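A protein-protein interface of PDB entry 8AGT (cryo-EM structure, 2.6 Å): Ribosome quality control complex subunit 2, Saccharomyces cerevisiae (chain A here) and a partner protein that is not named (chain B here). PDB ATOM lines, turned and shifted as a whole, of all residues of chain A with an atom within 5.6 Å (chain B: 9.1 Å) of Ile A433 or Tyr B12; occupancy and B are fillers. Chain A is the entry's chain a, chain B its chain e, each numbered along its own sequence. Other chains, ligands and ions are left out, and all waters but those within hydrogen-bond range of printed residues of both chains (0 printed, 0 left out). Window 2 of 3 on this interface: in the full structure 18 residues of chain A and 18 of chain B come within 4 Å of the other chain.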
ATOM      1  N   LEU A 398     -16.658 -18.113  -3.062  1.00  0.00           N
ATOM      2  CA  LEU A 398     -16.962 -18.357  -1.661  1.00  0.00           C
ATOM      3  C   LEU A 398     -15.728 -18.780  -0.884  1.00  0.00           C
ATOM      4  O   LEU A 398     -15.540 -18.362   0.253  1.00  0.00           O
ATOM      5  CB  LEU A 398     -18.133 -19.332  -1.473  1.00  0.00           C
ATOM      6  CG  LEU A 398     -18.073 -20.802  -1.884  1.00  0.00           C
ATOM      7  CD1 LEU A 398     -17.728 -21.684  -0.693  1.00  0.00           C
ATOM      8  CD2 LEU A 398     -19.411 -21.219  -2.471  1.00  0.00           C
ATOM      9  N   GLU A 401     -13.660 -15.875   0.210  1.00  0.00           N
ATOM     10  CA  GLU A 401     -14.247 -15.167   1.334  1.00  0.00           C
ATOM     11  C   GLU A 401     -13.954 -15.897   2.628  1.00  0.00           C
ATOM     12  O   GLU A 401     -13.629 -15.272   3.638  1.00  0.00           O
ATOM     13  CB  GLU A 401     -15.755 -15.055   1.159  1.00  0.00           C
ATOM     14  CG  GLU A 401     -16.182 -14.386  -0.132  1.00  0.00           C
ATOM     15  CD  GLU A 401     -17.595 -14.757  -0.531  1.00  0.00           C
ATOM     16  OE1 GLU A 401     -18.272 -15.452   0.256  1.00  0.00           O
ATOM     17  OE2 GLU A 401     -18.027 -14.362  -1.634  1.00  0.00           O
ATOM     18  N   VAL A 402     -14.056 -17.221   2.604  1.00  0.00           N
ATOM     19  CA  VAL A 402     -13.831 -17.993   3.814  1.00  0.00           C
ATOM     20  C   VAL A 402     -12.405 -17.793   4.286  1.00  0.00           C
ATOM     21  O   VAL A 402     -12.163 -17.563   5.470  1.00  0.00           O
ATOM     22  CB  VAL A 402     -14.069 -19.492   3.565  1.00  0.00           C
ATOM     23  CG1 VAL A 402     -13.710 -20.309   4.793  1.00  0.00           C
ATOM     24  CG2 VAL A 402     -15.514 -19.743   3.175  1.00  0.00           C
ATOM     25  N   ALA A 405     -11.800 -14.442   6.024  1.00  0.00           N
ATOM     26  CA  ALA A 405     -12.344 -14.368   7.361  1.00  0.00           C
ATOM     27  C   ALA A 405     -11.453 -15.073   8.369  1.00  0.00           C
ATOM     28  O   ALA A 405     -11.149 -14.525   9.431  1.00  0.00           O
ATOM     29  CB  ALA A 405     -13.735 -14.968   7.372  1.00  0.00           C
ATOM     30  N   ASN A 431     -24.251 -18.371  10.908  1.00  0.00           N
ATOM     31  CA  ASN A 431     -23.432 -17.656   9.941  1.00  0.00           C
ATOM     32  C   ASN A 431     -23.070 -18.624   8.828  1.00  0.00           C
ATOM     33  O   ASN A 431     -22.651 -19.751   9.091  1.00  0.00           O
ATOM     34  CB  ASN A 431     -22.167 -17.140  10.624  1.00  0.00           C
ATOM     35  CG  ASN A 431     -21.467 -16.054   9.832  1.00  0.00           C
ATOM     36  OD1 ASN A 431     -21.690 -15.895   8.634  1.00  0.00           O
ATOM     37  ND2 ASN A 431     -20.607 -15.300  10.506  1.00  0.00           N
ATOM     38  N   ARG A 432     -23.223 -18.189   7.583  1.00  0.00           N
ATOM     39  CA  ARG A 432     -22.963 -19.071   6.449  1.00  0.00           C
ATOM     40  C   ARG A 432     -21.519 -19.512   6.365  1.00  0.00           C
ATOM     41  O   ARG A 432     -21.229 -20.691   6.158  1.00  0.00           O
ATOM     42  CB  ARG A 432     -23.339 -18.345   5.159  1.00  0.00           C
ATOM     43  CG  ARG A 432     -23.042 -19.122   3.886  1.00  0.00           C
ATOM     44  CD  ARG A 432     -23.258 -18.274   2.641  1.00  0.00           C
ATOM     45  NE  ARG A 432     -22.169 -17.329   2.402  1.00  0.00           N
ATOM     46  CZ  ARG A 432     -22.161 -16.068   2.825  1.00  0.00           C
ATOM     47  NH1 ARG A 432     -23.184 -15.594   3.523  1.00  0.00           N
ATOM     48  NH2 ARG A 432     -21.127 -15.283   2.556  1.00  0.00           N
ATOM     49  N   ILE A 433     -20.604 -18.573   6.555  1.00  0.00           N
ATOM     50  CA  ILE A 433     -19.191 -18.894   6.446  1.00  0.00           C
ATOM     51  C   ILE A 433     -18.816 -19.892   7.526  1.00  0.00           C
ATOM     52  O   ILE A 433     -18.075 -20.842   7.277  1.00  0.00           O
ATOM     53  CB  ILE A 433     -18.327 -17.624   6.531  1.00  0.00           C
ATOM     54  CG1 ILE A 433     -18.771 -16.613   5.476  1.00  0.00           C
ATOM     55  CG2 ILE A 433     -16.861 -17.951   6.313  1.00  0.00           C
ATOM     56  CD1 ILE A 433     -18.451 -17.041   4.060  1.00  0.00           C
ATOM     57  N   ALA A 434     -19.357 -19.699   8.722  1.00  0.00           N
ATOM     58  CA  ALA A 434     -19.052 -20.596   9.822  1.00  0.00           C
ATOM     59  C   ALA A 434     -19.517 -21.998   9.493  1.00  0.00           C
ATOM     60  O   ALA A 434     -18.807 -22.965   9.755  1.00  0.00           O
ATOM     61  CB  ALA A 434     -19.720 -20.108  11.094  1.00  0.00           C
ATOM     62  N   GLN A 435     -20.689 -22.111   8.885  1.00  0.00           N
ATOM     63  CA  GLN A 435     -21.242 -23.421   8.570  1.00  0.00           C
ATOM     64  C   GLN A 435     -20.342 -24.177   7.622  1.00  0.00           C
ATOM     65  O   GLN A 435     -20.166 -25.384   7.762  1.00  0.00           O
ATOM     66  CB  GLN A 435     -22.613 -23.269   7.919  1.00  0.00           C
ATOM     67  CG  GLN A 435     -23.620 -22.479   8.732  1.00  0.00           C
ATOM     68  CD  GLN A 435     -24.861 -22.154   7.929  1.00  0.00           C
ATOM     69  OE1 GLN A 435     -24.871 -22.282   6.705  1.00  0.00           O
ATOM     70  NE2 GLN A 435     -25.915 -21.727   8.611  1.00  0.00           N
ATOM     71  N   LEU A 436     -19.763 -23.475   6.659  1.00  0.00           N
ATOM     72  CA  LEU A 436     -18.942 -24.141   5.660  1.00  0.00           C
ATOM     73  C   LEU A 436     -17.735 -24.850   6.253  1.00  0.00           C
ATOM     74  O   LEU A 436     -17.403 -25.957   5.841  1.00  0.00           O
ATOM     75  CB  LEU A 436     -18.474 -23.115   4.634  1.00  0.00           C
ATOM     76  CG  LEU A 436     -19.576 -22.467   3.797  1.00  0.00           C
ATOM     77  CD1 LEU A 436     -19.069 -21.226   3.082  1.00  0.00           C
ATOM     78  CD2 LEU A 436     -20.163 -23.466   2.813  1.00  0.00           C
ATOM     79  N   LEU A 437     -17.075 -24.225   7.217  1.00  0.00           N
ATOM     80  CA  LEU A 437     -15.866 -24.806   7.795  1.00  0.00           C
ATOM     81  C   LEU A 437     -16.060 -26.040   8.647  1.00  0.00           C
ATOM     82  O   LEU A 437     -16.985 -26.097   9.452  1.00  0.00           O
ATOM     83  CB  LEU A 437     -15.161 -23.758   8.647  1.00  0.00           C
ATOM     84  CG  LEU A 437     -14.487 -22.625   7.886  1.00  0.00           C
ATOM     85  CD1 LEU A 437     -14.149 -21.489   8.835  1.00  0.00           C
ATOM     86  CD2 LEU A 437     -13.241 -23.158   7.198  1.00  0.00           C
ATOM     87  N   ILE B   6      -9.327  -8.208  11.041  1.00  0.00           N
ATOM     88  CA  ILE B   6     -10.697  -7.711  10.945  1.00  0.00           C
ATOM     89  C   ILE B   6     -11.643  -8.744  11.529  1.00  0.00           C
ATOM     90  O   ILE B   6     -11.444  -9.941  11.326  1.00  0.00           O
ATOM     91  CB  ILE B   6     -11.083  -7.459   9.471  1.00  0.00           C
ATOM     92  CG1 ILE B   6     -10.230  -6.341   8.869  1.00  0.00           C
ATOM     93  CG2 ILE B   6     -12.551  -7.085   9.331  1.00  0.00           C
ATOM     94  CD1 ILE B   6     -10.510  -4.978   9.465  1.00  0.00           C
ATOM     95  N   ASN B   7     -12.664  -8.308  12.258  1.00  0.00           N
ATOM     96  CA  ASN B   7     -13.654  -9.247  12.764  1.00  0.00           C
ATOM     97  C   ASN B   7     -14.653  -9.485  11.656  1.00  0.00           C
ATOM     98  O   ASN B   7     -15.795  -9.038  11.738  1.00  0.00           O
ATOM     99  CB  ASN B   7     -14.360  -8.674  13.987  1.00  0.00           C
ATOM    100  CG  ASN B   7     -13.519  -8.766  15.244  1.00  0.00           C
ATOM    101  OD1 ASN B   7     -12.697  -9.669  15.389  1.00  0.00           O
ATOM    102  ND2 ASN B   7     -13.734  -7.839  16.171  1.00  0.00           N
ATOM    103  N   THR B   8     -14.232 -10.191  10.614  1.00  0.00           N
ATOM    104  CA  THR B   8     -15.099 -10.432   9.468  1.00  0.00           C
ATOM    105  C   THR B   8     -16.316 -11.254   9.848  1.00  0.00           C
ATOM    106  O   THR B   8     -17.420 -10.980   9.385  1.00  0.00           O
ATOM    107  CB  THR B   8     -14.334 -11.139   8.340  1.00  0.00           C
ATOM    108  OG1 THR B   8     -12.929 -10.909   8.494  1.00  0.00           O
ATOM    109  CG2 THR B   8     -14.784 -10.621   6.986  1.00  0.00           C
ATOM    110  N   PHE B   9     -16.123 -12.252  10.702  1.00  0.00           N
ATOM    111  CA  PHE B   9     -17.228 -13.110  11.099  1.00  0.00           C
ATOM    112  C   PHE B   9     -18.299 -12.299  11.801  1.00  0.00           C
ATOM    113  O   PHE B   9     -19.486 -12.523  11.589  1.00  0.00           O
ATOM    114  CB  PHE B   9     -16.743 -14.223  12.020  1.00  0.00           C
ATOM    115  CG  PHE B   9     -16.221 -15.421  11.293  1.00  0.00           C
ATOM    116  CD1 PHE B   9     -17.094 -16.353  10.764  1.00  0.00           C
ATOM    117  CD2 PHE B   9     -14.861 -15.618  11.137  1.00  0.00           C
ATOM    118  CE1 PHE B   9     -16.622 -17.461  10.092  1.00  0.00           C
ATOM    119  CE2 PHE B   9     -14.381 -16.725  10.468  1.00  0.00           C
ATOM    120  CZ  PHE B   9     -15.263 -17.647   9.941  1.00  0.00           C
ATOM    121  N   GLN B  10     -17.883 -11.362  12.643  1.00  0.00           N
ATOM    122  CA  GLN B  10     -18.841 -10.514  13.341  1.00  0.00           C
ATOM    123  C   GLN B  10     -19.639  -9.653  12.374  1.00  0.00           C
ATOM    124  O   GLN B  10     -20.833  -9.431  12.571  1.00  0.00           O
ATOM    125  CB  GLN B  10     -18.146  -9.659  14.400  1.00  0.00           C
ATOM    126  CG  GLN B  10     -17.324 -10.466  15.393  1.00  0.00           C
ATOM    127  CD  GLN B  10     -18.103 -11.609  16.020  1.00  0.00           C
ATOM    128  OE1 GLN B  10     -19.218 -11.427  16.509  1.00  0.00           O
ATOM    129  NE2 GLN B  10     -17.509 -12.794  16.017  1.00  0.00           N
ATOM    130  N   GLN B  11     -18.983  -9.153  11.335  1.00  0.00           N
ATOM    131  CA  GLN B  11     -19.691  -8.367  10.339  1.00  0.00           C
ATOM    132  C   GLN B  11     -20.749  -9.223   9.667  1.00  0.00           C
ATOM    133  O   GLN B  11     -21.856  -8.754   9.428  1.00  0.00           O
ATOM    134  CB  GLN B  11     -18.716  -7.821   9.303  1.00  0.00           C
ATOM    135  CG  GLN B  11     -17.708  -6.838   9.874  1.00  0.00           C
ATOM    136  CD  GLN B  11     -16.624  -6.470   8.881  1.00  0.00           C
ATOM    137  OE1 GLN B  11     -16.394  -7.180   7.903  1.00  0.00           O
ATOM    138  NE2 GLN B  11     -15.946  -5.356   9.133  1.00  0.00           N
ATOM    139  N   TYR B  12     -20.421 -10.473   9.359  1.00  0.00           N
ATOM    140  CA  TYR B  12     -21.410 -11.385   8.781  1.00  0.00           C
ATOM    141  C   TYR B  12     -22.535 -11.648   9.762  1.00  0.00           C
ATOM    142  O   TYR B  12     -23.694 -11.753   9.367  1.00  0.00           O
ATOM    143  CB  TYR B  12     -20.779 -12.722   8.399  1.00  0.00           C
ATOM    144  CG  TYR B  12     -19.714 -12.668   7.334  1.00  0.00           C
ATOM    145  CD1 TYR B  12     -19.936 -12.010   6.133  1.00  0.00           C
ATOM    146  CD2 TYR B  12     -18.499 -13.311   7.514  1.00  0.00           C
ATOM    147  CE1 TYR B  12     -18.963 -11.970   5.152  1.00  0.00           C
ATOM    148  CE2 TYR B  12     -17.520 -13.277   6.543  1.00  0.00           C
ATOM    149  CZ  TYR B  12     -17.757 -12.608   5.363  1.00  0.00           C
ATOM    150  OH  TYR B  12     -16.784 -12.574   4.390  1.00  0.00           O
ATOM    151  N   ASN B  13     -22.201 -11.768  11.042  1.00  0.00           N
ATOM    152  CA  ASN B  13     -23.201 -12.085  12.060  1.00  0.00           C
ATOM    153  C   ASN B  13     -24.282 -11.020  12.148  1.00  0.00           C
ATOM    154  O   ASN B  13     -25.448 -11.354  12.358  1.00  0.00           O
ATOM    155  CB  ASN B  13     -22.510 -12.238  13.419  1.00  0.00           C
ATOM    156  CG  ASN B  13     -23.367 -12.963  14.436  1.00  0.00           C
ATOM    157  OD1 ASN B  13     -24.271 -13.720  14.083  1.00  0.00           O
ATOM    158  ND2 ASN B  13     -23.073 -12.745  15.713  1.00  0.00           N
ATOM    159  N   THR B  14     -23.905  -9.748  12.033  1.00  0.00           N
ATOM    160  CA  THR B  14     -24.868  -8.633  12.097  1.00  0.00           C
ATOM    161  C   THR B  14     -25.687  -8.624  13.376  1.00  0.00           C
ATOM    162  O   THR B  14     -26.872  -8.291  13.352  1.00  0.00           O
ATOM    163  CB  THR B  14     -25.825  -8.542  10.876  1.00  0.00           C
ATOM    164  OG1 THR B  14     -26.816  -9.576  10.938  1.00  0.00           O
ATOM    165  CG2 THR B  14     -25.068  -8.628   9.562  1.00  0.00           C
ATOM    166  N   ASP B  15     -25.072  -8.986  14.494  1.00  0.00           N
ATOM    167  CA  ASP B  15     -25.777  -8.920  15.765  1.00  0.00           C
ATOM    168  C   ASP B  15     -25.006  -7.995  16.682  1.00  0.00           C
ATOM    169  O   ASP B  15     -23.802  -8.156  16.863  1.00  0.00           O
ATOM    170  CB  ASP B  15     -25.903 -10.305  16.395  1.00  0.00           C
ATOM    171  CG  ASP B  15     -26.766 -10.302  17.643  1.00  0.00           C
ATOM    172  OD1 ASP B  15     -27.605  -9.387  17.792  1.00  0.00           O
ATOM    173  OD2 ASP B  15     -26.611 -11.219  18.474  1.00  0.00           O
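ND2 of Asn A431 lies within hydrogen-bond range of O of Phe B9 (3.2 Å).
The side-chain hydroxyl (OG1) of Thr B8 lies within hydrogen-bond range of the backbone carbonyl oxygen (O) of Ile B6.
Among the printed residues, pairs that only touch across the chains: Ala A405 with Thr B8 (3.7 Å), Ala A405 with Phe B9 (3.6 Å), Asn A431 with Tyr B12 (3.3 Å), Asn A431 with Asn B13 (3.9 Å), Ile A433 with Phe B9 (3.8 Å), Ile A433 with Tyr B12 (3.7 Å) and Ala A434 with Phe B9 (3.8 Å).
No residue of chain B comes within 4 Å of Val A402.
Of the printed residues of chain B, Asn A431 touches Phe B9 (3.2 Å), Tyr B12 (3.3 Å) and Asn B13 (3.9 Å).
No residue of chain B comes within 4 Å of Arg A432.
Ile A433 touches two residues of chain B.
Of the printed residues of chain A, Thr B8 touches Ala A405.
Of the printed residues of chain A, Phe B9 touches Ala A405, Asn A431, Ile A433 and Ala A434.
Of chain A, only Asn A431 (3.3 Å) and Ile A433 (3.7 Å) come within 4 Å of Tyr B12.
Of the printed residues of chain A, Asn B13 touches Asn A431 (3.9 Å).
The nearest printed residue of chain A that does not touch Tyr B12 is Glu A401 (4.2 Å).
The nearest printed residue of chain A that does not touch Asn B13 is Arg A432 (7.4 Å).
Printed residues of chain B that touch a printed residue of chain A: Thr B8, Phe B9, Tyr B12 and Asn B13.
Of the 11 printed residues of chain A, 4 touch a printed residue of chain B.
Printed residues of chain A that touch a printed residue of chain B: Ala A405, Asn A431, Ile A433 and Ala A434.
Hydrophobic or aromatic side chains of chain A within 4 Å of the printed part of chain B: Ala A405 and Ile A433.
Among the printed residues, 8 pairs touch across the chains.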
